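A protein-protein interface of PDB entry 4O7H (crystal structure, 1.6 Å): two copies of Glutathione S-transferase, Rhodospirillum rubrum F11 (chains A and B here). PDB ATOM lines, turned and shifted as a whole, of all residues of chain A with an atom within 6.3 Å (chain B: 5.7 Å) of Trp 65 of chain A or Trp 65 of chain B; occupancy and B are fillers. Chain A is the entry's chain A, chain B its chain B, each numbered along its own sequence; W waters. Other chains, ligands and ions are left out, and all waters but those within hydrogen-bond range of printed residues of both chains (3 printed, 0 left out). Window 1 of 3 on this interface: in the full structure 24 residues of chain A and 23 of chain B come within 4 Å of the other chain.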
ATOM      1  N   ALA A  12      27.297  20.349 -33.636  1.00  0.00           N
ATOM      2  CA  ALA A  12      28.259  20.505 -32.580  1.00  0.00           C
ATOM      3  C   ALA A  12      29.425  21.394 -32.973  1.00  0.00           C
ATOM      4  O   ALA A  12      29.929  22.191 -32.196  1.00  0.00           O
ATOM      5  CB  ALA A  12      28.779  19.148 -32.145  1.00  0.00           C
ATOM      6  N   LYS A  15      28.334  24.926 -33.019  1.00  0.00           N
ATOM      7  CA  LYS A  15      28.320  25.419 -31.644  1.00  0.00           C
ATOM      8  C   LYS A  15      29.684  25.845 -31.141  1.00  0.00           C
ATOM      9  O   LYS A  15      29.843  26.893 -30.524  1.00  0.00           O
ATOM     10  CB  LYS A  15      27.676  24.417 -30.678  1.00  0.00           C
ATOM     11  CG  LYS A  15      28.083  24.711 -29.232  1.00  0.00           C
ATOM     12  CD  LYS A  15      27.194  24.077 -28.249  1.00  0.00           C
ATOM     13  CE  LYS A  15      27.253  22.608 -28.307  1.00  0.00           C
ATOM     14  NZ  LYS A  15      26.371  22.125 -27.217  1.00  0.00           N
ATOM     15  N   VAL A  16      30.713  25.036 -31.390  1.00  0.00           N
ATOM     16  CA  VAL A  16      32.043  25.387 -30.946  1.00  0.00           C
ATOM     17  C   VAL A  16      32.571  26.653 -31.653  1.00  0.00           C
ATOM     18  O   VAL A  16      33.163  27.518 -31.022  1.00  0.00           O
ATOM     19  CB  VAL A  16      32.996  24.187 -31.078  1.00  0.00           C
ATOM     20  CG1 VAL A  16      34.421  24.586 -30.717  1.00  0.00           C
ATOM     21  CG2 VAL A  16      32.602  23.040 -30.123  1.00  0.00           C
ATOM     22  N   THR A  62      38.541  16.683 -27.955  1.00  0.00           N
ATOM     23  CA  THR A  62      37.600  16.026 -28.864  1.00  0.00           C
ATOM     24  C   THR A  62      36.228  15.949 -28.165  1.00  0.00           C
ATOM     25  O   THR A  62      36.174  15.752 -26.943  1.00  0.00           O
ATOM     26  CB  THR A  62      38.151  14.616 -29.124  1.00  0.00           C
ATOM     27  OG1 THR A  62      39.421  14.701 -29.812  1.00  0.00           O
ATOM     28  CG2 THR A  62      37.221  13.813 -29.842  1.00  0.00           C
ATOM     29  N   ASP A  63      35.155  16.068 -28.930  1.00  0.00           N
ATOM     30  CA  ASP A  63      33.762  16.017 -28.508  1.00  0.00           C
ATOM     31  C   ASP A  63      33.287  17.427 -28.191  1.00  0.00           C
ATOM     32  O   ASP A  63      33.946  18.171 -27.466  1.00  0.00           O
ATOM     33  CB  ASP A  63      33.452  15.143 -27.267  1.00  0.00           C
ATOM     34  CG  ASP A  63      32.008  15.271 -26.840  1.00  0.00           C
ATOM     35  OD1 ASP A  63      31.131  14.809 -27.581  1.00  0.00           O
ATOM     36  OD2 ASP A  63      31.749  15.805 -25.755  1.00  0.00           O
ATOM     37  N   GLY A  64      32.144  17.800 -28.762  1.00  0.00           N
ATOM     38  CA  GLY A  64      31.592  19.142 -28.553  1.00  0.00           C
ATOM     39  C   GLY A  64      31.446  19.513 -27.080  1.00  0.00           C
ATOM     40  O   GLY A  64      31.780  20.635 -26.671  1.00  0.00           O
ATOM     41  N   TRP A  65      30.883  18.632 -26.269  1.00  0.00           N
ATOM     42  CA  TRP A  65      30.661  18.950 -24.895  1.00  0.00           C
ATOM     43  C   TRP A  65      31.993  19.077 -24.181  1.00  0.00           C
ATOM     44  O   TRP A  65      32.232  20.024 -23.412  1.00  0.00           O
ATOM     45  CB  TRP A  65      29.781  17.924 -24.188  1.00  0.00           C
ATOM     46  CG  TRP A  65      28.351  17.916 -24.558  1.00  0.00           C
ATOM     47  CD1 TRP A  65      27.697  18.683 -25.488  1.00  0.00           C
ATOM     48  CD2 TRP A  65      27.343  16.995 -24.027  1.00  0.00           C
ATOM     49  NE1 TRP A  65      26.337  18.306 -25.549  1.00  0.00           N
ATOM     50  CE2 TRP A  65      26.117  17.275 -24.690  1.00  0.00           C
ATOM     51  CE3 TRP A  65      27.384  15.935 -23.085  1.00  0.00           C
ATOM     52  CZ2 TRP A  65      24.931  16.589 -24.384  1.00  0.00           C
ATOM     53  CZ3 TRP A  65      26.256  15.297 -22.789  1.00  0.00           C
ATOM     54  CH2 TRP A  65      25.030  15.590 -23.443  1.00  0.00           C
ATOM     55  N   ALA A  66      32.905  18.111 -24.410  1.00  0.00           N
ATOM     56  CA  ALA A  66      34.218  18.210 -23.810  1.00  0.00           C
ATOM     57  C   ALA A  66      34.915  19.518 -24.160  1.00  0.00           C
ATOM     58  O   ALA A  66      35.532  20.165 -23.314  1.00  0.00           O
ATOM     59  CB  ALA A  66      35.098  17.067 -24.263  1.00  0.00           C
ATOM     60  N   ILE A  67      34.812  19.929 -25.426  1.00  0.00           N
ATOM     61  CA  ILE A  67      35.403  21.212 -25.852  1.00  0.00           C
ATOM     62  C   ILE A  67      34.747  22.388 -25.131  1.00  0.00           C
ATOM     63  O   ILE A  67      35.434  23.260 -24.621  1.00  0.00           O
ATOM     64  CB  ILE A  67      35.340  21.413 -27.386  1.00  0.00           C
ATOM     65  CG1 ILE A  67      36.241  20.382 -28.091  1.00  0.00           C
ATOM     66  CG2 ILE A  67      35.727  22.825 -27.732  1.00  0.00           C
ATOM     67  CD1 ILE A  67      35.937  20.270 -29.577  1.00  0.00           C
ATOM     68  N   CYS A  68      33.424  22.405 -25.061  1.00  0.00           N
ATOM     69  CA  CYS A  68      32.711  23.491 -24.378  1.00  0.00           C
ATOM     70  C   CYS A  68      33.060  23.591 -22.911  1.00  0.00           C
ATOM     71  O   CYS A  68      33.313  24.705 -22.389  1.00  0.00           O
ATOM     72  CB  CYS A  68      31.223  23.360 -24.609  1.00  0.00           C
ATOM     73  SG  CYS A  68      30.734  23.764 -26.318  1.00  0.00           S
ATOM     74  N   GLU A  69      33.171  22.456 -22.236  1.00  0.00           N
ATOM     75  CA  GLU A  69      33.511  22.496 -20.815  1.00  0.00           C
ATOM     76  C   GLU A  69      34.973  22.911 -20.649  1.00  0.00           C
ATOM     77  O   GLU A  69      35.291  23.694 -19.749  1.00  0.00           O
ATOM     78  CB  GLU A  69      33.272  21.150 -20.171  1.00  0.00           C
ATOM     79  CG  GLU A  69      31.824  20.711 -20.166  1.00  0.00           C
ATOM     80  CD  GLU A  69      30.970  21.523 -19.215  1.00  0.00           C
ATOM     81  OE1 GLU A  69      31.493  22.100 -18.247  1.00  0.00           O
ATOM     82  OE2 GLU A  69      29.767  21.563 -19.484  1.00  0.00           O
ATOM     83  N   TYR A  70      35.847  22.448 -21.545  1.00  0.00           N
ATOM     84  CA  TYR A  70      37.252  22.837 -21.549  1.00  0.00           C
ATOM     85  C   TYR A  70      37.343  24.340 -21.759  1.00  0.00           C
ATOM     86  O   TYR A  70      38.114  25.031 -21.050  1.00  0.00           O
ATOM     87  CB  TYR A  70      37.976  22.117 -22.679  1.00  0.00           C
ATOM     88  CG  TYR A  70      39.352  22.661 -22.967  1.00  0.00           C
ATOM     89  CD1 TYR A  70      40.462  22.236 -22.240  1.00  0.00           C
ATOM     90  CD2 TYR A  70      39.537  23.594 -23.979  1.00  0.00           C
ATOM     91  CE1 TYR A  70      41.757  22.739 -22.525  1.00  0.00           C
ATOM     92  CE2 TYR A  70      40.828  24.097 -24.246  1.00  0.00           C
ATOM     93  CZ  TYR A  70      41.897  23.687 -23.519  1.00  0.00           C
ATOM     94  OH  TYR A  70      43.186  24.212 -23.787  1.00  0.00           O
ATOM     95  N   LEU A  81      28.386  29.378 -19.208  1.00  0.00           N
ATOM     96  CA  LEU A  81      27.602  28.513 -18.298  1.00  0.00           C
ATOM     97  C   LEU A  81      26.906  29.264 -17.180  1.00  0.00           C
ATOM     98  O   LEU A  81      25.883  28.810 -16.692  1.00  0.00           O
ATOM     99  CB  LEU A  81      28.514  27.491 -17.670  1.00  0.00           C
ATOM    100  CG  LEU A  81      28.874  26.270 -18.521  1.00  0.00           C
ATOM    101  CD1 LEU A  81      30.022  25.510 -17.836  1.00  0.00           C
ATOM    102  CD2 LEU A  81      27.699  25.385 -18.820  1.00  0.00           C
ATOM    103  N   VAL A  91      21.445  25.401 -17.705  1.00  0.00           N
ATOM    104  CA  VAL A  91      22.135  25.498 -19.011  1.00  0.00           C
ATOM    105  C   VAL A  91      22.406  24.094 -19.563  1.00  0.00           C
ATOM    106  O   VAL A  91      22.129  23.794 -20.760  1.00  0.00           O
ATOM    107  CB  VAL A  91      23.448  26.280 -18.914  1.00  0.00           C
ATOM    108  CG1 VAL A  91      24.195  26.211 -20.247  1.00  0.00           C
ATOM    109  CG2 VAL A  91      23.178  27.724 -18.539  1.00  0.00           C
ATOM    110  N   ARG A  92      22.984  23.237 -18.735  1.00  0.00           N
ATOM    111  CA  ARG A  92      23.345  21.879 -19.174  1.00  0.00           C
ATOM    112  C   ARG A  92      22.119  21.013 -19.531  1.00  0.00           C
ATOM    113  O   ARG A  92      22.152  20.224 -20.518  1.00  0.00           O
ATOM    114  CB  ARG A  92      24.280  21.206 -18.174  1.00  0.00           C
ATOM    115  CG  ARG A  92      25.629  21.863 -18.086  1.00  0.00           C
ATOM    116  CD  ARG A  92      26.625  20.996 -17.381  1.00  0.00           C
ATOM    117  NE  ARG A  92      27.959  21.575 -17.206  1.00  0.00           N
ATOM    118  CZ  ARG A  92      28.426  22.146 -16.095  1.00  0.00           C
ATOM    119  NH1 ARG A  92      27.680  22.312 -15.013  1.00  0.00           N
ATOM    120  NH2 ARG A  92      29.668  22.537 -16.064  1.00  0.00           N
ATOM    121  N   ARG A  93      21.027  21.175 -18.772  1.00  0.00           N
ATOM    122  CA  ARG A  93      19.761  20.551 -19.098  1.00  0.00           C
ATOM    123  C   ARG A  93      19.329  20.909 -20.502  1.00  0.00           C
ATOM    124  O   ARG A  93      18.935  20.029 -21.271  1.00  0.00           O
ATOM    125  CB  ARG A  93      18.646  20.955 -18.071  1.00  0.00           C
ATOM    126  CG  ARG A  93      17.305  20.295 -18.360  1.00  0.00           C
ATOM    127  CD  ARG A  93      16.197  20.814 -17.430  1.00  0.00           C
ATOM    128  NE  ARG A  93      15.729  22.165 -17.760  1.00  0.00           N
ATOM    129  CZ  ARG A  93      14.874  22.408 -18.745  1.00  0.00           C
ATOM    130  NH1 ARG A  93      14.429  21.408 -19.510  1.00  0.00           N
ATOM    131  NH2 ARG A  93      14.487  23.646 -18.973  1.00  0.00           N
ATOM    132  N   VAL A  95      21.164  22.353 -22.934  1.00  0.00           N
ATOM    133  CA  VAL A  95      22.133  21.796 -23.903  1.00  0.00           C
ATOM    134  C   VAL A  95      21.734  20.379 -24.269  1.00  0.00           C
ATOM    135  O   VAL A  95      21.711  20.014 -25.458  1.00  0.00           O
ATOM    136  CB  VAL A  95      23.594  21.870 -23.379  1.00  0.00           C
ATOM    137  CG1 VAL A  95      24.531  21.059 -24.247  1.00  0.00           C
ATOM    138  CG2 VAL A  95      24.017  23.316 -23.370  1.00  0.00           C
ATOM    139  N   ALA A  96      21.484  19.534 -23.263  1.00  0.00           N
ATOM    140  CA  ALA A  96      21.055  18.166 -23.537  1.00  0.00           C
ATOM    141  C   ALA A  96      19.704  18.098 -24.269  1.00  0.00           C
ATOM    142  O   ALA A  96      19.528  17.239 -25.139  1.00  0.00           O
ATOM    143  CB  ALA A  96      20.965  17.368 -22.245  1.00  0.00           C
ATOM    144  N   ASP A  99      20.886  18.851 -27.830  1.00  0.00           N
ATOM    145  CA  ASP A  99      21.849  17.890 -28.426  1.00  0.00           C
ATOM    146  C   ASP A  99      21.377  16.420 -28.409  1.00  0.00           C
ATOM    147  O   ASP A  99      21.927  15.584 -29.133  1.00  0.00           O
ATOM    148  CB  ASP A  99      23.236  18.004 -27.774  1.00  0.00           C
ATOM    149  CG  ASP A  99      24.056  19.157 -28.295  1.00  0.00           C
ATOM    150  OD1 ASP A  99      23.838  19.687 -29.448  1.00  0.00           O
ATOM    151  OD2 ASP A  99      24.952  19.634 -27.543  1.00  0.00           O
ATOM    152  N   ARG A 100      20.389  16.092 -27.586  1.00  0.00           N
ATOM    153  CA  ARG A 100      19.726  14.773 -27.618  1.00  0.00           C
ATOM    154  C   ARG A 100      18.360  14.825 -28.279  1.00  0.00           C
ATOM    155  O   ARG A 100      18.154  14.160 -29.300  1.00  0.00           O
ATOM    156  CB  ARG A 100      19.593  14.162 -26.180  1.00  0.00           C
ATOM    157  CG  ARG A 100      18.767  12.885 -26.111  1.00  0.00           C
ATOM    158  CD  ARG A 100      18.903  12.110 -24.754  1.00  0.00           C
ATOM    159  NE  ARG A 100      18.537  12.995 -23.658  1.00  0.00           N
ATOM    160  CZ  ARG A 100      19.350  13.423 -22.698  1.00  0.00           C
ATOM    161  NH1 ARG A 100      20.618  13.035 -22.657  1.00  0.00           N
ATOM    162  NH2 ARG A 100      18.904  14.284 -21.821  1.00  0.00           N
ATOM    163  N   THR A 165      23.543  26.295 -28.567  1.00  0.00           N
ATOM    164  CA  THR A 165      23.215  24.942 -29.017  1.00  0.00           C
ATOM    165  C   THR A 165      21.888  24.949 -29.816  1.00  0.00           C
ATOM    166  O   THR A 165      21.833  24.463 -30.941  1.00  0.00           O
ATOM    167  CB  THR A 165      23.148  23.967 -27.822  1.00  0.00           C
ATOM    168  OG1 THR A 165      24.394  24.023 -27.083  1.00  0.00           O
ATOM    169  CG2 THR A 165      22.893  22.539 -28.325  1.00  0.00           C
ATOM    170  N   ASP B  63      18.965  15.541 -16.321  1.00  0.00           N
ATOM    171  CA  ASP B  63      19.914  15.091 -17.354  1.00  0.00           C
ATOM    172  C   ASP B  63      21.114  14.462 -16.641  1.00  0.00           C
ATOM    173  O   ASP B  63      21.701  15.071 -15.770  1.00  0.00           O
ATOM    174  CB  ASP B  63      20.446  16.173 -18.319  1.00  0.00           C
ATOM    175  CG  ASP B  63      21.554  15.640 -19.266  1.00  0.00           C
ATOM    176  OD1 ASP B  63      21.242  14.881 -20.163  1.00  0.00           O
ATOM    177  OD2 ASP B  63      22.736  16.060 -19.164  1.00  0.00           O
ATOM    178  N   GLY B  64      21.503  13.267 -17.090  1.00  0.00           N
ATOM    179  CA  GLY B  64      22.673  12.593 -16.532  1.00  0.00           C
ATOM    180  C   GLY B  64      23.974  13.396 -16.537  1.00  0.00           C
ATOM    181  O   GLY B  64      24.714  13.448 -15.580  1.00  0.00           O
ATOM    182  N   TRP B  65      24.264  14.052 -17.638  1.00  0.00           N
ATOM    183  CA  TRP B  65      25.463  14.789 -17.742  1.00  0.00           C
ATOM    184  C   TRP B  65      25.402  16.028 -16.829  1.00  0.00           C
ATOM    185  O   TRP B  65      26.338  16.330 -16.103  1.00  0.00           O
ATOM    186  CB  TRP B  65      25.694  15.136 -19.208  1.00  0.00           C
ATOM    187  CG  TRP B  65      26.692  16.075 -19.367  1.00  0.00           C
ATOM    188  CD1 TRP B  65      27.976  15.918 -18.992  1.00  0.00           C
ATOM    189  CD2 TRP B  65      26.604  17.379 -20.011  1.00  0.00           C
ATOM    190  NE1 TRP B  65      28.691  17.044 -19.295  1.00  0.00           N
ATOM    191  CE2 TRP B  65      27.871  17.950 -19.924  1.00  0.00           C
ATOM    192  CE3 TRP B  65      25.574  18.107 -20.623  1.00  0.00           C
ATOM    193  CZ2 TRP B  65      28.164  19.191 -20.453  1.00  0.00           C
ATOM    194  CZ3 TRP B  65      25.861  19.370 -21.104  1.00  0.00           C
ATOM    195  CH2 TRP B  65      27.138  19.887 -21.024  1.00  0.00           C
ATOM    196  N   ALA B  66      24.291  16.763 -16.866  1.00  0.00           N
ATOM    197  CA  ALA B  66      24.118  17.933 -15.991  1.00  0.00           C
ATOM    198  C   ALA B  66      24.278  17.506 -14.524  1.00  0.00           C
ATOM    199  O   ALA B  66      24.916  18.216 -13.752  1.00  0.00           O
ATOM    200  CB  ALA B  66      22.750  18.564 -16.207  1.00  0.00           C
ATOM    201  N   ILE B  67      23.718  16.351 -14.175  1.00  0.00           N
ATOM    202  CA  ILE B  67      23.825  15.831 -12.809  1.00  0.00           C
ATOM    203  C   ILE B  67      25.256  15.518 -12.477  1.00  0.00           C
ATOM    204  O   ILE B  67      25.754  15.942 -11.432  1.00  0.00           O
ATOM    205  CB  ILE B  67      22.905  14.626 -12.529  1.00  0.00           C
ATOM    206  CG1 ILE B  67      21.419  15.026 -12.600  1.00  0.00           C
ATOM    207  CG2 ILE B  67      23.263  14.024 -11.178  1.00  0.00           C
ATOM    208  CD1 ILE B  67      20.486  13.829 -12.722  1.00  0.00           C
ATOM    209  N   CYS B  68      25.974  14.849 -13.375  1.00  0.00           N
ATOM    210  CA  CYS B  68      27.390  14.527 -13.087  1.00  0.00           C
ATOM    211  C   CYS B  68      28.257  15.769 -12.926  1.00  0.00           C
ATOM    212  O   CYS B  68      29.123  15.819 -12.037  1.00  0.00           O
ATOM    213  CB  CYS B  68      27.915  13.598 -14.161  1.00  0.00           C
ATOM    214  SG  CYS B  68      27.235  11.915 -14.092  1.00  0.00           S
ATOM    215  N   GLU B  69      28.042  16.796 -13.774  1.00  0.00           N
ATOM    216  CA  GLU B  69      28.827  18.004 -13.670  1.00  0.00           C
ATOM    217  C   GLU B  69      28.466  18.747 -12.370  1.00  0.00           C
ATOM    218  O   GLU B  69      29.322  19.273 -11.715  1.00  0.00           O
ATOM    219  CB  GLU B  69      28.627  18.882 -14.893  1.00  0.00           C
ATOM    220  CG  GLU B  69      29.104  18.265 -16.224  1.00  0.00           C
ATOM    221  CD  GLU B  69      30.623  18.197 -16.370  1.00  0.00           C
ATOM    222  OE1 GLU B  69      31.365  18.799 -15.608  1.00  0.00           O
ATOM    223  OE2 GLU B  69      31.027  17.570 -17.359  1.00  0.00           O
ATOM    224  N   TYR B  70      27.176  18.730 -12.019  1.00  0.00           N
ATOM    225  CA  TYR B  70      26.702  19.356 -10.783  1.00  0.00           C
ATOM    226  C   TYR B  70      27.336  18.695  -9.597  1.00  0.00           C
ATOM    227  O   TYR B  70      27.849  19.393  -8.703  1.00  0.00           O
ATOM    228  CB  TYR B  70      25.192  19.224 -10.697  1.00  0.00           C
ATOM    229  CG  TYR B  70      24.582  19.544  -9.344  1.00  0.00           C
ATOM    230  CD1 TYR B  70      24.308  20.845  -8.966  1.00  0.00           C
ATOM    231  CD2 TYR B  70      24.329  18.519  -8.444  1.00  0.00           C
ATOM    232  CE1 TYR B  70      23.747  21.107  -7.693  1.00  0.00           C
ATOM    233  CE2 TYR B  70      23.763  18.796  -7.181  1.00  0.00           C
ATOM    234  CZ  TYR B  70      23.485  20.082  -6.859  1.00  0.00           C
ATOM    235  OH  TYR B  70      22.984  20.393  -5.579  1.00  0.00           O
ATOM    236  N   ARG B  92      35.896  13.415 -20.443  1.00  0.00           N
ATOM    237  CA  ARG B  92      34.681  13.843 -21.132  1.00  0.00           C
ATOM    238  C   ARG B  92      34.632  13.262 -22.563  1.00  0.00           C
ATOM    239  O   ARG B  92      33.557  12.871 -23.034  1.00  0.00           O
ATOM    240  CB  ARG B  92      34.533  15.357 -21.105  1.00  0.00           C
ATOM    241  CG  ARG B  92      34.253  15.906 -19.703  1.00  0.00           C
ATOM    242  CD  ARG B  92      33.794  17.349 -19.751  1.00  0.00           C
ATOM    243  NE  ARG B  92      33.527  17.949 -18.433  1.00  0.00           N
ATOM    244  CZ  ARG B  92      34.358  18.777 -17.802  1.00  0.00           C
ATOM    245  NH1 ARG B  92      35.527  19.126 -18.299  1.00  0.00           N
ATOM    246  NH2 ARG B  92      33.973  19.323 -16.649  1.00  0.00           N
ATOM    247  N   VAL B  95      33.509   9.682 -21.932  1.00  0.00           N
ATOM    248  CA  VAL B  95      32.094   9.703 -21.580  1.00  0.00           C
ATOM    249  C   VAL B  95      31.251   9.805 -22.841  1.00  0.00           C
ATOM    250  O   VAL B  95      30.296   9.030 -23.041  1.00  0.00           O
ATOM    251  CB  VAL B  95      31.776  10.855 -20.609  1.00  0.00           C
ATOM    252  CG1 VAL B  95      30.256  11.106 -20.525  1.00  0.00           C
ATOM    253  CG2 VAL B  95      32.317  10.553 -19.253  1.00  0.00           C
HETATM  254  O   HOH W   1      25.281  21.025 -14.122  1.00  0.00           O
HETATM  255  O   HOH W   2      36.701  18.967 -21.034  1.00  0.00           O
HETATM  256  O   HOH W   3      31.322  14.530 -23.325  1.00  0.00           O
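Water W3 bridges OD2 of Asp 63 of chain A (2.8 Å) and O of Arg 92 of chain B (2.8 Å).
Water W2 bridges the backbone carbonyl oxygen (O) of Ala 66 of chain A and the guanidinium group (NH1) of Arg 92 of chain B.
Water W1 lies within hydrogen-bond range of O of Ala 66 of chain B (2.9 Å) and NH1 of Arg 92 of chain A (2.9 Å).
Trp 65 of chain B touches its own counterpart, Trp 65 of chain A.
Ala 66 of chain A touches Arg 92 of chain B, and with the chains exchanged Arg 92 of chain A touches Ala 66 of chain B.
Arg 92 of chain A touches Trp 65 of chain B, but with the chains exchanged Trp 65 of chain A does not touch Arg 92 of chain B (4.8 Å).
Val 95 of chain A touches Trp 65 of chain B, but with the chains exchanged Trp 65 of chain A does not touch Val 95 of chain B (6.2 Å).
Of the 10 pairs that touch across the chains among the printed residues, 5 have their exchanged pair printed and touching as well.
Among the printed residues, merely in contact across the chains: Trp 65 of chain A with Trp 65 of chain B (3.5 Å), Ala 66 of chain A with Arg 92 of chain B (3.6 Å), Glu 69 of chain A with Trp 65 of chain B (3.0 Å), Glu 69 of chain A with Arg 92 of chain B (3.5 Å), Arg 92 of chain A with Trp 65 of chain B (3.8 Å), Arg 92 of chain A with Ala 66 of chain B (3.6 Å), Arg 92 of chain A with Glu 69 of chain B (3.5 Å), Val 95 of chain A with Trp 65 of chain B (3.8 Å) and Ala 96 of chain A with Asp 63 of chain B (3.3 Å).
OD1 of Asp 63 of chain B is in salt-bridge range of NH2 of Arg 100 of chain A (2.9 Å).
Trp 65 of chain A touches just one residue of chain B: Trp 65.
Trp 65 of chain B touches four residues of chain A.
Of the printed residues of chain A, Glu 69 of chain B touches Arg 92.
Printed residues of chain A within 4 Å of Arg 92 of chain B: Ala 66 and Glu 69.
Of the printed residues of chain B, Ala 96 of chain A touches Asp 63 (3.3 Å).
Asp 63 of chain A touches none of the printed residues of chain B.
The indole nitrogen of Trp 65 of chain A is in hydrogen-bond range of the side-chain carboxylate of Asp 99 of chain A (2.8 Å).
The guanidinium group of Arg 92 of chain B is in salt-bridge range of the side-chain carboxylate of Glu 69 of chain B, 2.7 Å away.
N of Trp 65 of chain A is in hydrogen-bond range of OD2 of Asp 63 of chain A (3.0 Å).
The side-chain carboxylate (OD2) of Asp 63 of chain A sits at hydrogen-bond distance from the backbone NH (N) of Ala 66 of chain A (2.9 Å).
The side-chain carboxylate of Asp 63 of chain B lies within hydrogen-bond range of the backbone NH of Ala 66 of chain B (2.9 Å).
The backbone NH of Trp 65 of chain B lies within hydrogen-bond range of the side-chain carboxylate of Asp 63 of chain B.
Of the 10 printed residues of chain B, 5 touch a printed residue of chain A.
Hydrophobic or aromatic side chains of chain A within 4 Å of the printed part of chain B: Trp 65, Ala 66, Val 95 and Ala 96.
Among the printed residues, 10 pairs touch across the chains.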
